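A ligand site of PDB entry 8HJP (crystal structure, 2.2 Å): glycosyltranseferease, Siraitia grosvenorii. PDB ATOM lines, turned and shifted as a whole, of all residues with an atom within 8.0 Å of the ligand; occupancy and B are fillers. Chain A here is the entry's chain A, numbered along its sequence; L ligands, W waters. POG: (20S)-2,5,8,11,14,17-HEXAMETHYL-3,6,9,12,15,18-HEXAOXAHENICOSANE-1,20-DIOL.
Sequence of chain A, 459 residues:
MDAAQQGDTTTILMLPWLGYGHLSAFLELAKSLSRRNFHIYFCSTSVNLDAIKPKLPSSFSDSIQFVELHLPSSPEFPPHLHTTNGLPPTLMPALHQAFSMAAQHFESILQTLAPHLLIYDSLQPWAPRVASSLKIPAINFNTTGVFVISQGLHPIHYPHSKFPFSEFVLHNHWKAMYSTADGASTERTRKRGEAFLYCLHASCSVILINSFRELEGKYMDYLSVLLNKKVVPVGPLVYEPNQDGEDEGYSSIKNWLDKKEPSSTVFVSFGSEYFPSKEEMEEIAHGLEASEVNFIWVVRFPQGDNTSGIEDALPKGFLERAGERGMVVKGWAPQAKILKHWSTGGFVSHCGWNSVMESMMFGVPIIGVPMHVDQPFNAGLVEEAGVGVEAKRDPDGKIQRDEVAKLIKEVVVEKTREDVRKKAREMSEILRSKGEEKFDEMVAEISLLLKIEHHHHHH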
ATOM      1  N   HIS A 154      17.837   5.879 -11.127  1.00  0.00           N
ATOM      2  CA  HIS A 154      16.673   5.027 -11.361  1.00  0.00           C
ATOM      3  C   HIS A 154      16.289   4.177 -10.153  1.00  0.00           C
ATOM      4  O   HIS A 154      15.084   4.073  -9.871  1.00  0.00           O
ATOM      5  CB  HIS A 154      16.907   4.128 -12.592  1.00  0.00           C
ATOM      6  CG  HIS A 154      15.938   2.995 -12.678  1.00  0.00           C
ATOM      7  ND1 HIS A 154      14.687   3.124 -13.229  1.00  0.00           N
ATOM      8  CD2 HIS A 154      16.026   1.708 -12.256  1.00  0.00           C
ATOM      9  CE1 HIS A 154      14.049   1.970 -13.165  1.00  0.00           C
ATOM     10  NE2 HIS A 154      14.845   1.095 -12.583  1.00  0.00           N
ATOM     11  N   HIS A 157      13.827   5.811  -7.262  1.00  0.00           N
ATOM     12  CA  HIS A 157      12.374   5.900  -7.473  1.00  0.00           C
ATOM     13  C   HIS A 157      11.808   4.506  -7.778  1.00  0.00           C
ATOM     14  O   HIS A 157      10.625   4.290  -7.490  1.00  0.00           O
ATOM     15  CB  HIS A 157      12.136   6.952  -8.561  1.00  0.00           C
ATOM     16  CG  HIS A 157      12.762   8.270  -8.280  1.00  0.00           C
ATOM     17  ND1 HIS A 157      13.995   8.615  -8.773  1.00  0.00           N
ATOM     18  CD2 HIS A 157      12.339   9.331  -7.567  1.00  0.00           C
ATOM     19  CE1 HIS A 157      14.322   9.825  -8.376  1.00  0.00           C
ATOM     20  NE2 HIS A 157      13.312  10.290  -7.632  1.00  0.00           N
ATOM     21  N   TYR A 158      12.632   3.607  -8.303  1.00  0.00           N
ATOM     22  CA  TYR A 158      12.151   2.258  -8.681  1.00  0.00           C
ATOM     23  C   TYR A 158      13.091   1.185  -8.139  1.00  0.00           C
ATOM     24  O   TYR A 158      13.851   0.608  -8.919  1.00  0.00           O
ATOM     25  CB  TYR A 158      12.036   2.149 -10.204  1.00  0.00           C
ATOM     26  CG  TYR A 158      11.052   3.104 -10.806  1.00  0.00           C
ATOM     27  CD1 TYR A 158       9.700   2.853 -10.731  1.00  0.00           C
ATOM     28  CD2 TYR A 158      11.463   4.263 -11.436  1.00  0.00           C
ATOM     29  CE1 TYR A 158       8.771   3.726 -11.281  1.00  0.00           C
ATOM     30  CE2 TYR A 158      10.560   5.150 -11.979  1.00  0.00           C
ATOM     31  CZ  TYR A 158       9.205   4.877 -11.908  1.00  0.00           C
ATOM     32  OH  TYR A 158       8.288   5.724 -12.447  1.00  0.00           O
ATOM     33  N   HIS A 160      12.602  -1.844  -7.261  1.00  0.00           N
ATOM     34  CA  HIS A 160      12.302  -3.215  -7.756  1.00  0.00           C
ATOM     35  C   HIS A 160      12.204  -3.300  -9.274  1.00  0.00           C
ATOM     36  O   HIS A 160      12.505  -4.368  -9.806  1.00  0.00           O
ATOM     37  CB  HIS A 160      10.923  -3.578  -7.207  1.00  0.00           C
ATOM     38  CG  HIS A 160       9.877  -2.588  -7.592  1.00  0.00           C
ATOM     39  ND1 HIS A 160       8.905  -2.858  -8.533  1.00  0.00           N
ATOM     40  CD2 HIS A 160       9.683  -1.301  -7.212  1.00  0.00           C
ATOM     41  CE1 HIS A 160       8.145  -1.798  -8.696  1.00  0.00           C
ATOM     42  NE2 HIS A 160       8.608  -0.826  -7.906  1.00  0.00           N
ATOM     43  N   SER A 161      11.780  -2.218  -9.947  1.00  0.00           N
ATOM     44  CA  SER A 161      11.547  -2.266 -11.421  1.00  0.00           C
ATOM     45  C   SER A 161      12.836  -2.274 -12.253  1.00  0.00           C
ATOM     46  O   SER A 161      13.898  -1.915 -11.712  1.00  0.00           O
ATOM     47  CB  SER A 161      10.649  -1.166 -11.839  1.00  0.00           C
ATOM     48  OG  SER A 161      11.435  -0.116 -12.372  1.00  0.00           O
ATOM     49  N   LYS A 162      12.726  -2.656 -13.533  1.00  0.00           N
ATOM     50  CA  LYS A 162      13.893  -2.786 -14.433  1.00  0.00           C
ATOM     51  C   LYS A 162      14.276  -1.434 -15.028  1.00  0.00           C
ATOM     52  O   LYS A 162      13.374  -0.640 -15.277  1.00  0.00           O
ATOM     53  CB  LYS A 162      13.581  -3.747 -15.577  1.00  0.00           C
ATOM     54  CG  LYS A 162      14.747  -4.225 -16.424  1.00  0.00           C
ATOM     55  CD  LYS A 162      14.318  -5.211 -17.484  1.00  0.00           C
ATOM     56  CE  LYS A 162      15.459  -6.002 -18.070  1.00  0.00           C
ATOM     57  NZ  LYS A 162      14.960  -7.071 -18.979  1.00  0.00           N
ATOM     58  N   PHE A 163      15.576  -1.215 -15.245  1.00  0.00           N
ATOM     59  CA  PHE A 163      15.996   0.014 -15.895  1.00  0.00           C
ATOM     60  C   PHE A 163      15.492   0.012 -17.341  1.00  0.00           C
ATOM     61  O   PHE A 163      15.726  -0.960 -18.070  1.00  0.00           O
ATOM     62  CB  PHE A 163      17.515   0.179 -15.857  1.00  0.00           C
ATOM     63  CG  PHE A 163      18.001   1.469 -16.485  1.00  0.00           C
ATOM     64  CD1 PHE A 163      18.038   2.640 -15.747  1.00  0.00           C
ATOM     65  CD2 PHE A 163      18.443   1.491 -17.798  1.00  0.00           C
ATOM     66  CE1 PHE A 163      18.483   3.822 -16.318  1.00  0.00           C
ATOM     67  CE2 PHE A 163      18.901   2.676 -18.368  1.00  0.00           C
ATOM     68  CZ  PHE A 163      18.918   3.839 -17.625  1.00  0.00           C
ATOM     69  N   PRO A 164      14.797   1.046 -17.780  1.00  0.00           N
ATOM     70  CA  PRO A 164      14.235   1.074 -19.131  1.00  0.00           C
ATOM     71  C   PRO A 164      15.325   1.351 -20.165  1.00  0.00           C
ATOM     72  O   PRO A 164      16.387   1.878 -19.840  1.00  0.00           O
ATOM     73  CB  PRO A 164      13.235   2.225 -19.070  1.00  0.00           C
ATOM     74  CG  PRO A 164      13.886   3.154 -18.107  1.00  0.00           C
ATOM     75  CD  PRO A 164      14.426   2.258 -17.023  1.00  0.00           C
ATOM     76  N   PHE A 165      15.062   0.952 -21.395  1.00  0.00           N
ATOM     77  CA  PHE A 165      15.850   1.292 -22.583  1.00  0.00           C
ATOM     78  C   PHE A 165      17.262   0.732 -22.571  1.00  0.00           C
ATOM     79  O   PHE A 165      18.076   1.148 -23.403  1.00  0.00           O
ATOM     80  CB  PHE A 165      15.934   2.817 -22.871  1.00  0.00           C
ATOM     81  CG  PHE A 165      14.713   3.644 -22.527  1.00  0.00           C
ATOM     82  CD1 PHE A 165      13.441   3.216 -22.901  1.00  0.00           C
ATOM     83  CD2 PHE A 165      14.822   4.819 -21.787  1.00  0.00           C
ATOM     84  CE1 PHE A 165      12.316   3.971 -22.572  1.00  0.00           C
ATOM     85  CE2 PHE A 165      13.698   5.558 -21.450  1.00  0.00           C
ATOM     86  CZ  PHE A 165      12.449   5.136 -21.845  1.00  0.00           C
ATOM     87  N   GLY A 217      19.947  10.050 -26.293  1.00  0.00           N
ATOM     88  CA  GLY A 217      18.729  10.848 -26.250  1.00  0.00           C
ATOM     89  C   GLY A 217      17.651  10.275 -25.352  1.00  0.00           C
ATOM     90  O   GLY A 217      17.002  10.998 -24.601  1.00  0.00           O
ATOM     91  N   LYS A 218      17.435   8.945 -25.415  1.00  0.00           N
ATOM     92  CA  LYS A 218      16.448   8.323 -24.535  1.00  0.00           C
ATOM     93  C   LYS A 218      16.810   8.521 -23.066  1.00  0.00           C
ATOM     94  O   LYS A 218      15.952   8.843 -22.239  1.00  0.00           O
ATOM     95  CB  LYS A 218      16.336   6.822 -24.821  1.00  0.00           C
ATOM     96  CG  LYS A 218      15.790   6.450 -26.193  1.00  0.00           C
ATOM     97  CD  LYS A 218      15.923   4.947 -26.381  1.00  0.00           C
ATOM     98  CE  LYS A 218      17.301   4.446 -25.942  1.00  0.00           C
ATOM     99  NZ  LYS A 218      17.502   3.008 -26.225  1.00  0.00           N
ATOM    100  N   TYR A 219      18.091   8.339 -22.734  1.00  0.00           N
ATOM    101  CA  TYR A 219      18.543   8.525 -21.359  1.00  0.00           C
ATOM    102  C   TYR A 219      18.412   9.984 -20.925  1.00  0.00           C
ATOM    103  O   TYR A 219      18.126  10.255 -19.751  1.00  0.00           O
ATOM    104  CB  TYR A 219      19.979   8.013 -21.229  1.00  0.00           C
ATOM    105  CG  TYR A 219      20.138   6.610 -21.779  1.00  0.00           C
ATOM    106  CD1 TYR A 219      19.264   5.598 -21.408  1.00  0.00           C
ATOM    107  CD2 TYR A 219      21.144   6.303 -22.679  1.00  0.00           C
ATOM    108  CE1 TYR A 219      19.396   4.314 -21.913  1.00  0.00           C
ATOM    109  CE2 TYR A 219      21.290   5.028 -23.196  1.00  0.00           C
ATOM    110  CZ  TYR A 219      20.405   4.030 -22.810  1.00  0.00           C
ATOM    111  OH  TYR A 219      20.542   2.759 -23.317  1.00  0.00           O
ATOM    112  N   MET A 220      18.642  10.931 -21.834  1.00  0.00           N
ATOM    113  CA  MET A 220      18.493  12.335 -21.482  1.00  0.00           C
ATOM    114  C   MET A 220      17.051  12.663 -21.120  1.00  0.00           C
ATOM    115  O   MET A 220      16.797  13.429 -20.179  1.00  0.00           O
ATOM    116  CB  MET A 220      18.934  13.239 -22.632  1.00  0.00           C
ATOM    117  CG  MET A 220      20.417  13.226 -22.937  1.00  0.00           C
ATOM    118  SD  MET A 220      20.739  14.242 -24.385  1.00  0.00           S
ATOM    119  CE  MET A 220      22.402  13.726 -24.791  1.00  0.00           C
ATOM    120  N   ASP A 221      16.096  12.111 -21.863  1.00  0.00           N
ATOM    121  CA  ASP A 221      14.689  12.323 -21.552  1.00  0.00           C
ATOM    122  C   ASP A 221      14.361  11.739 -20.186  1.00  0.00           C
ATOM    123  O   ASP A 221      13.678  12.382 -19.365  1.00  0.00           O
ATOM    124  CB  ASP A 221      13.814  11.697 -22.628  1.00  0.00           C
ATOM    125  CG  ASP A 221      13.989  12.352 -23.979  1.00  0.00           C
ATOM    126  OD1 ASP A 221      14.448  13.518 -24.019  1.00  0.00           O
ATOM    127  OD2 ASP A 221      13.692  11.698 -24.998  1.00  0.00           O
ATOM    128  N   TYR A 222      14.826  10.521 -19.924  1.00  0.00           N
ATOM    129  CA  TYR A 222      14.586   9.892 -18.630  1.00  0.00           C
ATOM    130  C   TYR A 222      15.278  10.656 -17.505  1.00  0.00           C
ATOM    131  O   TYR A 222      14.689  10.866 -16.445  1.00  0.00           O
ATOM    132  CB  TYR A 222      15.051   8.436 -18.664  1.00  0.00           C
ATOM    133  CG  TYR A 222      14.663   7.633 -17.440  1.00  0.00           C
ATOM    134  CD1 TYR A 222      13.475   7.893 -16.759  1.00  0.00           C
ATOM    135  CD2 TYR A 222      15.466   6.593 -16.982  1.00  0.00           C
ATOM    136  CE1 TYR A 222      13.118   7.161 -15.635  1.00  0.00           C
ATOM    137  CE2 TYR A 222      15.111   5.852 -15.862  1.00  0.00           C
ATOM    138  CZ  TYR A 222      13.934   6.136 -15.200  1.00  0.00           C
ATOM    139  OH  TYR A 222      13.579   5.402 -14.093  1.00  0.00           O
ATOM    140  N   LEU A 223      16.536  11.085 -17.726  1.00  0.00           N
ATOM    141  CA  LEU A 223      17.240  11.828 -16.691  1.00  0.00           C
ATOM    142  C   LEU A 223      16.511  13.103 -16.293  1.00  0.00           C
ATOM    143  O   LEU A 223      16.475  13.468 -15.115  1.00  0.00           O
ATOM    144  CB  LEU A 223      18.661  12.161 -17.161  1.00  0.00           C
ATOM    145  CG  LEU A 223      19.471  12.957 -16.133  1.00  0.00           C
ATOM    146  CD1 LEU A 223      19.694  12.153 -14.863  1.00  0.00           C
ATOM    147  CD2 LEU A 223      20.797  13.418 -16.719  1.00  0.00           C
ATOM    148  N   SER A 224      15.923  13.800 -17.279  1.00  0.00           N
ATOM    149  CA  SER A 224      15.216  15.038 -16.956  1.00  0.00           C
ATOM    150  C   SER A 224      14.055  14.755 -16.011  1.00  0.00           C
ATOM    151  O   SER A 224      13.818  15.494 -15.053  1.00  0.00           O
ATOM    152  CB  SER A 224      14.721  15.744 -18.208  1.00  0.00           C
ATOM    153  OG  SER A 224      13.919  16.867 -17.863  1.00  0.00           O
ATOM    154  N   VAL A 225      13.322  13.673 -16.266  1.00  0.00           N
ATOM    155  CA  VAL A 225      12.203  13.284 -15.408  1.00  0.00           C
ATOM    156  C   VAL A 225      12.731  12.972 -14.012  1.00  0.00           C
ATOM    157  O   VAL A 225      12.189  13.439 -13.004  1.00  0.00           O
ATOM    158  CB  VAL A 225      11.444  12.082 -16.001  1.00  0.00           C
ATOM    159  CG1 VAL A 225      10.430  11.541 -15.000  1.00  0.00           C
ATOM    160  CG2 VAL A 225      10.772  12.462 -17.306  1.00  0.00           C
ATOM    161  N   LEU A 226      13.772  12.142 -13.941  1.00  0.00           N
ATOM    162  CA  LEU A 226      14.347  11.780 -12.650  1.00  0.00           C
ATOM    163  C   LEU A 226      14.780  13.011 -11.863  1.00  0.00           C
ATOM    164  O   LEU A 226      14.590  13.073 -10.638  1.00  0.00           O
ATOM    165  CB  LEU A 226      15.523  10.824 -12.852  1.00  0.00           C
ATOM    166  CG  LEU A 226      15.157   9.441 -13.400  1.00  0.00           C
ATOM    167  CD1 LEU A 226      16.399   8.714 -13.884  1.00  0.00           C
ATOM    168  CD2 LEU A 226      14.424   8.633 -12.349  1.00  0.00           C
HETATM  169  OH  POG L   1      10.148   0.509 -15.074  1.00  0.00           O
HETATM  170  C2  POG L   1       9.422   1.352 -14.213  1.00  0.00           C
HETATM  171  C1  POG L   1       8.173   0.664 -13.664  1.00  0.00           C
HETATM  172  C3  POG L   1       8.932   2.579 -14.954  1.00  0.00           C
HETATM  173  O2  POG L   1       9.852   3.600 -14.718  1.00  0.00           O
HETATM  174  C5  POG L   1      10.034   4.411 -15.831  1.00  0.00           C
HETATM  175  O4  POG L   1      11.765   7.434 -25.395  1.00  0.00           O
HETATM  176  C9  POG L   1      11.708   7.667 -24.014  1.00  0.00           C
HETATM  177  C10 POG L   1      10.760   8.827 -23.743  1.00  0.00           C
HETATM  178  O5  POG L   1      10.759   9.151 -22.380  1.00  0.00           O
HETATM  179  C11 POG L   1      10.526   8.087 -21.513  1.00  0.00           C
HETATM  180  C12 POG L   1      10.787   8.514 -20.070  1.00  0.00           C
HETATM  181  O6  POG L   1      10.221   7.561 -19.198  1.00  0.00           O
HETATM  182  C13 POG L   1       9.220   7.985 -18.300  1.00  0.00           C
HETATM  183  C14 POG L   1       9.256   7.111 -17.048  1.00  0.00           C
HETATM  184  O7  POG L   1       8.809   5.817 -17.359  1.00  0.00           O
HETATM  185  C15 POG L   1       8.673   4.966 -16.259  1.00  0.00           C
HETATM  186  C16 POG L   1      10.616   3.570 -16.966  1.00  0.00           C
HETATM  187  C17 POG L   1       8.369   7.722 -15.970  1.00  0.00           C
HETATM  188  C18 POG L   1      10.229   9.922 -19.852  1.00  0.00           C
HETATM  189  C19 POG L   1       9.352   8.420 -24.176  1.00  0.00           C
HETATM  190  O   HOH W   1       8.887   8.108 -12.710  1.00  0.00           O
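The side-chain hydroxyl of Ser 161 sits at hydrogen-bond distance from an oxygen (OH) of the ligand.
OH of Tyr 158 lies close to O2 of the ligand (3.5 Å).
An oxygen (OH) of the ligand is in hydrogen-bond range of the backbone carbonyl oxygen of Lys 162 (3.4 Å).
O of Ser 161 lies within hydrogen-bond range of NE2 of His 154 (3.3 Å).
O of Phe 165 lies within hydrogen-bond range of NZ of Lys 218, at 3.4 Å.
O of Phe 165 lies within hydrogen-bond range of OH of Tyr 219 (2.9 Å).
Pro 164 touches the ligand.
Phe 165 touches the ligand (CZ to C9, 3.4 Å).
Asp 221 touches the ligand.
Val 225 touches the ligand.
Hydrophobic or aromatic side chains that line the ligand: Tyr 158, Pro 164, Phe 165 and Val 225.
Of the 19 residues printed, 7 come within 4 Å of the ligand.
The nearest printed residue that does not touch the ligand is Tyr 222 (4.1 Å).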
